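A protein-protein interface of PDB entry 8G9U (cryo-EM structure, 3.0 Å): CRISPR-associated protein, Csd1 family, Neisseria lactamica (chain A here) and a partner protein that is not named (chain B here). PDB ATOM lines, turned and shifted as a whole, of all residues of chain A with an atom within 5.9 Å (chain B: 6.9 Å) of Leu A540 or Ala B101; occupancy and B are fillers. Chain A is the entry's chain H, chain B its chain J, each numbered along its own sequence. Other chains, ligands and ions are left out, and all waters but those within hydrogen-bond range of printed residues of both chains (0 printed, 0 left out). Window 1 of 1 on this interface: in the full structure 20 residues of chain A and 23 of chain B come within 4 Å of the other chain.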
ATOM      1  N   VAL A 470      -5.839  21.298   4.785  1.00  0.00           N
ATOM      2  CA  VAL A 470      -4.961  21.716   5.865  1.00  0.00           C
ATOM      3  C   VAL A 470      -3.633  22.187   5.315  1.00  0.00           C
ATOM      4  O   VAL A 470      -3.001  23.065   5.892  1.00  0.00           O
ATOM      5  CB  VAL A 470      -4.783  20.599   6.899  1.00  0.00           C
ATOM      6  CG1 VAL A 470      -6.120  20.258   7.485  1.00  0.00           C
ATOM      7  CG2 VAL A 470      -4.140  19.396   6.285  1.00  0.00           C
ATOM      8  N   LEU A 471      -3.192  21.649   4.187  1.00  0.00           N
ATOM      9  CA  LEU A 471      -2.010  22.221   3.564  1.00  0.00           C
ATOM     10  C   LEU A 471      -2.303  23.535   2.873  1.00  0.00           C
ATOM     11  O   LEU A 471      -1.404  24.363   2.755  1.00  0.00           O
ATOM     12  CB  LEU A 471      -1.379  21.243   2.593  1.00  0.00           C
ATOM     13  CG  LEU A 471      -0.560  20.168   3.291  1.00  0.00           C
ATOM     14  CD1 LEU A 471      -1.370  19.149   4.036  1.00  0.00           C
ATOM     15  CD2 LEU A 471       0.209  19.502   2.257  1.00  0.00           C
ATOM     16  N   LEU A 474      -1.919  25.663   5.744  1.00  0.00           N
ATOM     17  CA  LEU A 474      -0.501  25.750   6.044  1.00  0.00           C
ATOM     18  C   LEU A 474       0.179  26.732   5.122  1.00  0.00           C
ATOM     19  O   LEU A 474       1.013  27.525   5.550  1.00  0.00           O
ATOM     20  CB  LEU A 474       0.133  24.378   5.902  1.00  0.00           C
ATOM     21  CG  LEU A 474       1.547  24.221   6.401  1.00  0.00           C
ATOM     22  CD1 LEU A 474       1.467  23.949   7.839  1.00  0.00           C
ATOM     23  CD2 LEU A 474       2.169  23.060   5.721  1.00  0.00           C
ATOM     24  N   PHE A 509       6.395  21.960   0.553  1.00  0.00           N
ATOM     25  CA  PHE A 509       6.201  22.134   1.985  1.00  0.00           C
ATOM     26  C   PHE A 509       7.328  21.561   2.816  1.00  0.00           C
ATOM     27  O   PHE A 509       7.438  21.902   3.995  1.00  0.00           O
ATOM     28  CB  PHE A 509       4.892  21.503   2.409  1.00  0.00           C
ATOM     29  CG  PHE A 509       3.722  22.351   2.116  1.00  0.00           C
ATOM     30  CD1 PHE A 509       3.583  23.565   2.729  1.00  0.00           C
ATOM     31  CD2 PHE A 509       2.776  21.952   1.213  1.00  0.00           C
ATOM     32  CE1 PHE A 509       2.514  24.355   2.461  1.00  0.00           C
ATOM     33  CE2 PHE A 509       1.705  22.742   0.941  1.00  0.00           C
ATOM     34  CZ  PHE A 509       1.573  23.946   1.566  1.00  0.00           C
ATOM     35  N   GLY A 510       8.162  20.703   2.244  1.00  0.00           N
ATOM     36  CA  GLY A 510       9.388  20.364   2.922  1.00  0.00           C
ATOM     37  C   GLY A 510      10.414  21.470   2.886  1.00  0.00           C
ATOM     38  O   GLY A 510      11.410  21.389   3.602  1.00  0.00           O
ATOM     39  N   MET A 513       8.878  25.184   4.824  1.00  0.00           N
ATOM     40  CA  MET A 513       8.915  25.165   6.264  1.00  0.00           C
ATOM     41  C   MET A 513      10.331  25.152   6.788  1.00  0.00           C
ATOM     42  O   MET A 513      10.531  25.044   7.999  1.00  0.00           O
ATOM     43  CB  MET A 513       8.111  23.980   6.753  1.00  0.00           C
ATOM     44  CG  MET A 513       6.676  24.211   6.388  1.00  0.00           C
ATOM     45  SD  MET A 513       5.595  22.889   6.818  1.00  0.00           S
ATOM     46  CE  MET A 513       5.661  23.148   8.553  1.00  0.00           C
ATOM     47  N   GLU A 535      -0.363  28.619  15.311  1.00  0.00           N
ATOM     48  CA  GLU A 535      -1.435  28.204  14.425  1.00  0.00           C
ATOM     49  C   GLU A 535      -0.914  27.340  13.306  1.00  0.00           C
ATOM     50  O   GLU A 535      -1.669  26.545  12.756  1.00  0.00           O
ATOM     51  CB  GLU A 535      -2.172  29.366  13.810  1.00  0.00           C
ATOM     52  CG  GLU A 535      -1.392  30.015  12.759  1.00  0.00           C
ATOM     53  CD  GLU A 535      -2.245  30.895  11.930  1.00  0.00           C
ATOM     54  OE1 GLU A 535      -3.474  30.884  12.138  1.00  0.00           O
ATOM     55  OE2 GLU A 535      -1.690  31.592  11.072  1.00  0.00           O
ATOM     56  N   ILE A 536       0.355  27.473  12.935  1.00  0.00           N
ATOM     57  CA  ILE A 536       0.855  26.541  11.945  1.00  0.00           C
ATOM     58  C   ILE A 536       1.081  25.180  12.569  1.00  0.00           C
ATOM     59  O   ILE A 536       0.919  24.170  11.891  1.00  0.00           O
ATOM     60  CB  ILE A 536       2.099  27.101  11.238  1.00  0.00           C
ATOM     61  CG1 ILE A 536       2.420  26.240  10.052  1.00  0.00           C
ATOM     62  CG2 ILE A 536       3.293  27.027  12.103  1.00  0.00           C
ATOM     63  CD1 ILE A 536       3.371  26.863   9.145  1.00  0.00           C
ATOM     64  N   ARG A 537       1.360  25.126  13.870  1.00  0.00           N
ATOM     65  CA  ARG A 537       1.317  23.864  14.593  1.00  0.00           C
ATOM     66  C   ARG A 537      -0.082  23.277  14.592  1.00  0.00           C
ATOM     67  O   ARG A 537      -0.250  22.068  14.442  1.00  0.00           O
ATOM     68  CB  ARG A 537       1.780  24.050  16.030  1.00  0.00           C
ATOM     69  CG  ARG A 537       3.245  24.193  16.185  1.00  0.00           C
ATOM     70  CD  ARG A 537       3.556  24.831  17.492  1.00  0.00           C
ATOM     71  NE  ARG A 537       2.583  24.444  18.494  1.00  0.00           N
ATOM     72  CZ  ARG A 537       2.230  25.224  19.499  1.00  0.00           C
ATOM     73  NH1 ARG A 537       2.781  26.416  19.618  1.00  0.00           N
ATOM     74  NH2 ARG A 537       1.332  24.814  20.378  1.00  0.00           N
ATOM     75  N   GLN A 538      -1.094  24.112  14.812  1.00  0.00           N
ATOM     76  CA  GLN A 538      -2.463  23.615  14.805  1.00  0.00           C
ATOM     77  C   GLN A 538      -2.847  23.115  13.425  1.00  0.00           C
ATOM     78  O   GLN A 538      -3.412  22.029  13.276  1.00  0.00           O
ATOM     79  CB  GLN A 538      -3.424  24.704  15.255  1.00  0.00           C
ATOM     80  CG  GLN A 538      -3.042  25.334  16.544  1.00  0.00           C
ATOM     81  CD  GLN A 538      -3.090  24.366  17.690  1.00  0.00           C
ATOM     82  OE1 GLN A 538      -2.242  24.398  18.575  1.00  0.00           O
ATOM     83  NE2 GLN A 538      -4.088  23.495  17.689  1.00  0.00           N
ATOM     84  N   ILE A 539      -2.538  23.906  12.404  1.00  0.00           N
ATOM     85  CA  ILE A 539      -2.790  23.517  11.027  1.00  0.00           C
ATOM     86  C   ILE A 539      -2.136  22.188  10.739  1.00  0.00           C
ATOM     87  O   ILE A 539      -2.743  21.281  10.164  1.00  0.00           O
ATOM     88  CB  ILE A 539      -2.248  24.587  10.075  1.00  0.00           C
ATOM     89  CG1 ILE A 539      -3.176  25.778  10.031  1.00  0.00           C
ATOM     90  CG2 ILE A 539      -2.073  24.014   8.723  1.00  0.00           C
ATOM     91  CD1 ILE A 539      -2.597  26.895   9.286  1.00  0.00           C
ATOM     92  N   LEU A 540      -0.889  22.054  11.149  1.00  0.00           N
ATOM     93  CA  LEU A 540      -0.081  20.935  10.741  1.00  0.00           C
ATOM     94  C   LEU A 540      -0.322  19.735  11.640  1.00  0.00           C
ATOM     95  O   LEU A 540       0.123  18.629  11.329  1.00  0.00           O
ATOM     96  CB  LEU A 540       1.368  21.386  10.776  1.00  0.00           C
ATOM     97  CG  LEU A 540       2.290  20.421  10.114  1.00  0.00           C
ATOM     98  CD1 LEU A 540       1.795  20.495   8.706  1.00  0.00           C
ATOM     99  CD2 LEU A 540       3.671  20.911  10.191  1.00  0.00           C
ATOM    100  N   GLU A 541      -1.034  19.942  12.745  1.00  0.00           N
ATOM    101  CA  GLU A 541      -1.507  18.846  13.571  1.00  0.00           C
ATOM    102  C   GLU A 541      -2.549  18.023  12.836  1.00  0.00           C
ATOM    103  O   GLU A 541      -2.627  16.806  13.027  1.00  0.00           O
ATOM    104  CB  GLU A 541      -2.067  19.411  14.875  1.00  0.00           C
ATOM    105  CG  GLU A 541      -3.152  18.587  15.517  1.00  0.00           C
ATOM    106  CD  GLU A 541      -3.642  19.190  16.815  1.00  0.00           C
ATOM    107  OE1 GLU A 541      -4.404  18.516  17.537  1.00  0.00           O
ATOM    108  OE2 GLU A 541      -3.269  20.342  17.115  1.00  0.00           O
ATOM    109  N   HIS A 542      -3.347  18.661  11.989  1.00  0.00           N
ATOM    110  CA  HIS A 542      -4.263  17.937  11.127  1.00  0.00           C
ATOM    111  C   HIS A 542      -3.554  17.245   9.980  1.00  0.00           C
ATOM    112  O   HIS A 542      -4.185  16.461   9.267  1.00  0.00           O
ATOM    113  CB  HIS A 542      -5.317  18.882  10.566  1.00  0.00           C
ATOM    114  CG  HIS A 542      -5.973  19.732  11.600  1.00  0.00           C
ATOM    115  ND1 HIS A 542      -6.437  19.224  12.792  1.00  0.00           N
ATOM    116  CD2 HIS A 542      -6.246  21.056  11.622  1.00  0.00           C
ATOM    117  CE1 HIS A 542      -6.966  20.199  13.507  1.00  0.00           C
ATOM    118  NE2 HIS A 542      -6.862  21.322  12.820  1.00  0.00           N
ATOM    119  N   CYS A 543      -2.273  17.516   9.783  1.00  0.00           N
ATOM    120  CA  CYS A 543      -1.503  16.934   8.697  1.00  0.00           C
ATOM    121  C   CYS A 543      -0.611  15.841   9.260  1.00  0.00           C
ATOM    122  O   CYS A 543       0.181  16.093  10.168  1.00  0.00           O
ATOM    123  CB  CYS A 543      -0.665  17.999   7.998  1.00  0.00           C
ATOM    124  SG  CYS A 543       0.277  17.395   6.604  1.00  0.00           S
ATOM    125  N   GLN A 544      -0.745  14.632   8.729  1.00  0.00           N
ATOM    126  CA  GLN A 544       0.134  13.545   9.125  1.00  0.00           C
ATOM    127  C   GLN A 544       1.300  13.359   8.176  1.00  0.00           C
ATOM    128  O   GLN A 544       2.307  12.763   8.565  1.00  0.00           O
ATOM    129  CB  GLN A 544      -0.648  12.232   9.223  1.00  0.00           C
ATOM    130  CG  GLN A 544      -1.443  12.107  10.498  1.00  0.00           C
ATOM    131  CD  GLN A 544      -0.614  12.424  11.723  1.00  0.00           C
ATOM    132  OE1 GLN A 544       0.519  11.964  11.857  1.00  0.00           O
ATOM    133  NE2 GLN A 544      -1.176  13.218  12.625  1.00  0.00           N
ATOM    134  N   PHE A 546       2.765  15.506   4.329  1.00  0.00           N
ATOM    135  CA  PHE A 546       2.500  16.206   3.093  1.00  0.00           C
ATOM    136  C   PHE A 546       2.345  15.167   1.994  1.00  0.00           C
ATOM    137  O   PHE A 546       3.181  14.266   1.885  1.00  0.00           O
ATOM    138  CB  PHE A 546       3.626  17.175   2.775  1.00  0.00           C
ATOM    139  CG  PHE A 546       3.845  18.183   3.842  1.00  0.00           C
ATOM    140  CD1 PHE A 546       2.784  18.859   4.381  1.00  0.00           C
ATOM    141  CD2 PHE A 546       5.100  18.440   4.323  1.00  0.00           C
ATOM    142  CE1 PHE A 546       2.972  19.776   5.364  1.00  0.00           C
ATOM    143  CE2 PHE A 546       5.289  19.361   5.312  1.00  0.00           C
ATOM    144  CZ  PHE A 546       4.223  20.027   5.829  1.00  0.00           C
ATOM    145  N   GLY B   1      -2.577  15.123  17.443  1.00  0.00           N
ATOM    146  CA  GLY B   1      -1.881  15.180  16.172  1.00  0.00           C
ATOM    147  C   GLY B   1      -0.389  14.958  16.287  1.00  0.00           C
ATOM    148  O   GLY B   1       0.403  15.754  15.805  1.00  0.00           O
ATOM    149  N   GLY B  10      12.036  10.851   9.006  1.00  0.00           N
ATOM    150  CA  GLY B  10      11.793  12.275   8.911  1.00  0.00           C
ATOM    151  C   GLY B  10      10.932  12.780  10.047  1.00  0.00           C
ATOM    152  O   GLY B  10      11.233  13.802  10.655  1.00  0.00           O
ATOM    153  N   TYR B  11       9.864  12.055  10.367  1.00  0.00           N
ATOM    154  CA  TYR B  11       8.955  12.492  11.419  1.00  0.00           C
ATOM    155  C   TYR B  11       9.613  12.403  12.784  1.00  0.00           C
ATOM    156  O   TYR B  11       9.460  13.303  13.613  1.00  0.00           O
ATOM    157  CB  TYR B  11       7.667  11.676  11.349  1.00  0.00           C
ATOM    158  CG  TYR B  11       6.517  12.163  12.198  1.00  0.00           C
ATOM    159  CD1 TYR B  11       6.511  13.402  12.747  1.00  0.00           C
ATOM    160  CD2 TYR B  11       5.379  11.417  12.329  1.00  0.00           C
ATOM    161  CE1 TYR B  11       5.444  13.842  13.498  1.00  0.00           C
ATOM    162  CE2 TYR B  11       4.313  11.842  13.059  1.00  0.00           C
ATOM    163  CZ  TYR B  11       4.349  13.060  13.641  1.00  0.00           C
ATOM    164  OH  TYR B  11       3.275  13.495  14.370  1.00  0.00           O
ATOM    165  N   GLY B  14      11.975  15.286  12.970  1.00  0.00           N
ATOM    166  CA  GLY B  14      11.250  16.515  13.202  1.00  0.00           C
ATOM    167  C   GLY B  14      10.833  16.642  14.646  1.00  0.00           C
ATOM    168  O   GLY B  14      10.959  17.702  15.252  1.00  0.00           O
ATOM    169  N   PHE B  40      17.513  24.503  11.392  1.00  0.00           N
ATOM    170  CA  PHE B  40      16.367  23.791  10.830  1.00  0.00           C
ATOM    171  C   PHE B  40      16.543  23.528   9.343  1.00  0.00           C
ATOM    172  O   PHE B  40      16.149  22.472   8.844  1.00  0.00           O
ATOM    173  CB  PHE B  40      15.082  24.585  11.068  1.00  0.00           C
ATOM    174  CG  PHE B  40      13.824  23.808  10.809  1.00  0.00           C
ATOM    175  CD1 PHE B  40      13.452  23.457   9.536  1.00  0.00           C
ATOM    176  CD2 PHE B  40      12.989  23.472  11.844  1.00  0.00           C
ATOM    177  CE1 PHE B  40      12.310  22.752   9.310  1.00  0.00           C
ATOM    178  CE2 PHE B  40      11.837  22.773  11.611  1.00  0.00           C
ATOM    179  CZ  PHE B  40      11.499  22.418  10.342  1.00  0.00           C
ATOM    180  N   SER B  44      16.156  19.610   8.634  1.00  0.00           N
ATOM    181  CA  SER B  44      15.092  19.090   7.803  1.00  0.00           C
ATOM    182  C   SER B  44      15.612  18.376   6.574  1.00  0.00           C
ATOM    183  O   SER B  44      14.910  17.521   6.036  1.00  0.00           O
ATOM    184  CB  SER B  44      14.172  20.227   7.378  1.00  0.00           C
ATOM    185  OG  SER B  44      13.144  19.755   6.534  1.00  0.00           O
ATOM    186  N   LEU B  92      17.649  13.539   4.315  1.00  0.00           N
ATOM    187  CA  LEU B  92      16.263  13.154   4.521  1.00  0.00           C
ATOM    188  C   LEU B  92      15.575  12.965   3.182  1.00  0.00           C
ATOM    189  O   LEU B  92      15.655  13.827   2.304  1.00  0.00           O
ATOM    190  CB  LEU B  92      15.527  14.194   5.354  1.00  0.00           C
ATOM    191  CG  LEU B  92      15.485  13.892   6.845  1.00  0.00           C
ATOM    192  CD1 LEU B  92      14.615  14.860   7.596  1.00  0.00           C
ATOM    193  CD2 LEU B  92      14.987  12.503   7.051  1.00  0.00           C
ATOM    194  N   GLN B  96      10.336  12.173   3.731  1.00  0.00           N
ATOM    195  CA  GLN B  96      10.885  12.470   5.037  1.00  0.00           C
ATOM    196  C   GLN B  96      11.244  13.937   5.153  1.00  0.00           C
ATOM    197  O   GLN B  96      11.220  14.493   6.251  1.00  0.00           O
ATOM    198  CB  GLN B  96      12.107  11.600   5.279  1.00  0.00           C
ATOM    199  CG  GLN B  96      11.928  10.079   5.376  1.00  0.00           C
ATOM    200  CD  GLN B  96      10.511   9.552   5.529  1.00  0.00           C
ATOM    201  OE1 GLN B  96       9.620  10.199   6.063  1.00  0.00           O
ATOM    202  NE2 GLN B  96      10.301   8.343   5.032  1.00  0.00           N
ATOM    203  N   GLN B  97      11.584  14.574   4.033  1.00  0.00           N
ATOM    204  CA  GLN B  97      11.802  16.015   4.044  1.00  0.00           C
ATOM    205  C   GLN B  97      10.606  16.712   4.650  1.00  0.00           C
ATOM    206  O   GLN B  97      10.735  17.479   5.609  1.00  0.00           O
ATOM    207  CB  GLN B  97      11.980  16.544   2.619  1.00  0.00           C
ATOM    208  CG  GLN B  97      13.368  16.759   2.082  1.00  0.00           C
ATOM    209  CD  GLN B  97      14.363  17.113   3.120  1.00  0.00           C
ATOM    210  OE1 GLN B  97      15.405  16.483   3.211  1.00  0.00           O
ATOM    211  NE2 GLN B  97      14.030  18.071   3.965  1.00  0.00           N
ATOM    212  N   GLY B  98       9.426  16.445   4.100  1.00  0.00           N
ATOM    213  CA  GLY B  98       8.225  17.073   4.616  1.00  0.00           C
ATOM    214  C   GLY B  98       7.851  16.581   5.998  1.00  0.00           C
ATOM    215  O   GLY B  98       7.415  17.362   6.851  1.00  0.00           O
ATOM    216  N   LEU B  99       8.001  15.280   6.235  1.00  0.00           N
ATOM    217  CA  LEU B  99       7.672  14.742   7.541  1.00  0.00           C
ATOM    218  C   LEU B  99       8.552  15.311   8.636  1.00  0.00           C
ATOM    219  O   LEU B  99       8.171  15.257   9.798  1.00  0.00           O
ATOM    220  CB  LEU B  99       7.766  13.226   7.540  1.00  0.00           C
ATOM    221  CG  LEU B  99       6.459  12.576   7.117  1.00  0.00           C
ATOM    222  CD1 LEU B  99       6.713  11.520   6.093  1.00  0.00           C
ATOM    223  CD2 LEU B  99       5.770  11.979   8.312  1.00  0.00           C
ATOM    224  N   PHE B 100       9.721  15.852   8.308  1.00  0.00           N
ATOM    225  CA  PHE B 100      10.495  16.527   9.340  1.00  0.00           C
ATOM    226  C   PHE B 100       9.786  17.780   9.816  1.00  0.00           C
ATOM    227  O   PHE B 100       9.740  18.058  11.011  1.00  0.00           O
ATOM    228  CB  PHE B 100      11.886  16.876   8.835  1.00  0.00           C
ATOM    229  CG  PHE B 100      12.746  17.525   9.869  1.00  0.00           C
ATOM    230  CD1 PHE B 100      12.601  18.862  10.172  1.00  0.00           C
ATOM    231  CD2 PHE B 100      13.697  16.801  10.539  1.00  0.00           C
ATOM    232  CE1 PHE B 100      13.378  19.451  11.112  1.00  0.00           C
ATOM    233  CE2 PHE B 100      14.479  17.394  11.482  1.00  0.00           C
ATOM    234  CZ  PHE B 100      14.322  18.722  11.762  1.00  0.00           C
ATOM    235  N   ALA B 101       9.280  18.582   8.891  1.00  0.00           N
ATOM    236  CA  ALA B 101       8.517  19.752   9.297  1.00  0.00           C
ATOM    237  C   ALA B 101       7.257  19.332  10.029  1.00  0.00           C
ATOM    238  O   ALA B 101       6.861  19.953  11.025  1.00  0.00           O
ATOM    239  CB  ALA B 101       8.185  20.592   8.075  1.00  0.00           C
ATOM    240  N   ILE B 102       6.631  18.256   9.556  1.00  0.00           N
ATOM    241  CA  ILE B 102       5.507  17.665  10.271  1.00  0.00           C
ATOM    242  C   ILE B 102       5.907  17.351  11.699  1.00  0.00           C
ATOM    243  O   ILE B 102       5.186  17.664  12.641  1.00  0.00           O
ATOM    244  CB  ILE B 102       5.019  16.396   9.558  1.00  0.00           C
ATOM    245  CG1 ILE B 102       4.535  16.724   8.166  1.00  0.00           C
ATOM    246  CG2 ILE B 102       3.900  15.775  10.330  1.00  0.00           C
ATOM    247  CD1 ILE B 102       3.433  17.660   8.192  1.00  0.00           C
ATOM    248  N   GLY B 103       7.054  16.708  11.875  1.00  0.00           N
ATOM    249  CA  GLY B 103       7.482  16.324  13.203  1.00  0.00           C
ATOM    250  C   GLY B 103       7.811  17.507  14.071  1.00  0.00           C
ATOM    251  O   GLY B 103       7.439  17.550  15.239  1.00  0.00           O
ATOM    252  N   TYR B 104       8.514  18.478  13.511  1.00  0.00           N
ATOM    253  CA  TYR B 104       8.790  19.692  14.245  1.00  0.00           C
ATOM    254  C   TYR B 104       7.512  20.278  14.799  1.00  0.00           C
ATOM    255  O   TYR B 104       7.414  20.546  15.996  1.00  0.00           O
ATOM    256  CB  TYR B 104       9.505  20.691  13.352  1.00  0.00           C
ATOM    257  CG  TYR B 104       9.823  21.949  14.079  1.00  0.00           C
ATOM    258  CD1 TYR B 104      10.846  22.007  14.990  1.00  0.00           C
ATOM    259  CD2 TYR B 104       9.084  23.081  13.858  1.00  0.00           C
ATOM    260  CE1 TYR B 104      11.118  23.162  15.655  1.00  0.00           C
ATOM    261  CE2 TYR B 104       9.351  24.229  14.513  1.00  0.00           C
ATOM    262  CZ  TYR B 104      10.361  24.270  15.408  1.00  0.00           C
ATOM    263  OH  TYR B 104      10.605  25.451  16.055  1.00  0.00           O
ATOM    264  N   TYR B 105       6.493  20.414  13.972  1.00  0.00           N
ATOM    265  CA  TYR B 105       5.322  21.109  14.476  1.00  0.00           C
ATOM    266  C   TYR B 105       4.380  20.212  15.263  1.00  0.00           C
ATOM    267  O   TYR B 105       3.748  20.690  16.205  1.00  0.00           O
ATOM    268  CB  TYR B 105       4.627  21.811  13.325  1.00  0.00           C
ATOM    269  CG  TYR B 105       5.398  23.052  12.999  1.00  0.00           C
ATOM    270  CD1 TYR B 105       5.599  24.012  13.958  1.00  0.00           C
ATOM    271  CD2 TYR B 105       6.018  23.214  11.785  1.00  0.00           C
ATOM    272  CE1 TYR B 105       6.314  25.127  13.705  1.00  0.00           C
ATOM    273  CE2 TYR B 105       6.756  24.334  11.519  1.00  0.00           C
ATOM    274  CZ  TYR B 105       6.899  25.290  12.490  1.00  0.00           C
ATOM    275  OH  TYR B 105       7.636  26.425  12.265  1.00  0.00           O
ATOM    276  N   HIS B 106       4.339  18.918  14.974  1.00  0.00           N
ATOM    277  CA  HIS B 106       3.609  17.974  15.804  1.00  0.00           C
ATOM    278  C   HIS B 106       4.188  17.919  17.205  1.00  0.00           C
ATOM    279  O   HIS B 106       3.465  18.080  18.191  1.00  0.00           O
ATOM    280  CB  HIS B 106       3.667  16.592  15.171  1.00  0.00           C
ATOM    281  CG  HIS B 106       2.678  16.388  14.074  1.00  0.00           C
ATOM    282  ND1 HIS B 106       1.850  15.291  14.017  1.00  0.00           N
ATOM    283  CD2 HIS B 106       2.366  17.151  13.006  1.00  0.00           C
ATOM    284  CE1 HIS B 106       1.086  15.375  12.946  1.00  0.00           C
ATOM    285  NE2 HIS B 106       1.377  16.497  12.316  1.00  0.00           N
ATOM    286  N   GLU B 107       5.494  17.698  17.313  1.00  0.00           N
ATOM    287  CA  GLU B 107       6.115  17.606  18.623  1.00  0.00           C
ATOM    288  C   GLU B 107       6.150  18.958  19.304  1.00  0.00           C
ATOM    289  O   GLU B 107       6.082  19.038  20.530  1.00  0.00           O
ATOM    290  CB  GLU B 107       7.519  17.038  18.497  1.00  0.00           C
ATOM    291  CG  GLU B 107       8.206  16.801  19.811  1.00  0.00           C
ATOM    292  CD  GLU B 107       7.897  15.439  20.378  1.00  0.00           C
ATOM    293  OE1 GLU B 107       7.629  14.509  19.593  1.00  0.00           O
ATOM    294  OE2 GLU B 107       7.921  15.288  21.611  1.00  0.00           O
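The backbone carbonyl oxygen (O) of Ser B44 lies close to the side-chain amide oxygen (OE1) of Gln B97 (3.1 Å). The side-chain amide nitrogen (NE2) of Gln A538 sits at hydrogen-bond distance from the side-chain carboxylate (OE2) of Glu A541 (3.3 Å).
Of the printed residues of chain B, Leu A540 touches Ala B101, Ile B102, Tyr B105 and His B106. Of the printed residues of chain B, Cys A543 touches Ile B102 and His B106. Gly B14 touches none of the printed residues of chain A. Of the printed residues of chain A, Tyr B105 touches Met A513, Ile A536, Arg A537 and Leu A540. Glu B107 touches none of the printed residues of chain A. The nearest printed residue of chain B that does not touch Phe A546 is Ala B101 (4.2 Å).
Printed residues of chain B that touch a printed residue of chain A: Gly B1, Tyr B11, Phe B40, Ser B44, Gly B98, Leu B99, Ala B101, Ile B102, Tyr B105 and His B106. Hydrophobic or aromatic side chains of chain A that line the printed part of chain B: Met A513, Ile A536, Leu A540 and Phe A546. Among the printed residues, 21 pairs touch across the chains. Among the printed residues, no Asp or Glu carboxylate lies within 4 Å of a Lys or Arg side-chain nitrogen of the other chain.
Among the printed residues, merely in contact across the chains: Gly A510 with Ser B44 (3.8 Å), Gly A510 with Gly B98 (3.9 Å), Met A513 with Phe B40 (3.2 Å), Met A513 with Ala B101 (3.6 Å), Met A513 with Tyr B105 (3.3 Å), Ile A536 with Tyr B105 (3.9 Å), Arg A537 with Tyr B105 (3.2 Å), Leu A540 with Ala B101 (3.4 Å), Leu A540 with Ile B102 (3.3 Å), Leu A540 with Tyr B105 (3.4 Å), Glu A541 with Gly B1 (3.6 Å), Glu A541 with His B106 (3.9 Å), Cys A543 with Ile B102 (3.5 Å), Gln A544 with Tyr B11 (3.98 Å), Gln A544 with Leu B99 (3.6 Å), Gln A544 with Ile B102 (3.8 Å), Gln A544 with His B106 (3.1 Å), Phe A546 with Gly B98 (3.3 Å) and Phe A546 with Ile B102 (3.4 Å).
NE2 of His B106 lies within hydrogen-bond range of O of Cys A543, at 2.5 Å. A ring nitrogen (NE2) of His B106 lies within hydrogen-bond range of the backbone carbonyl oxygen (O) of Leu A540, at 2.7 Å.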
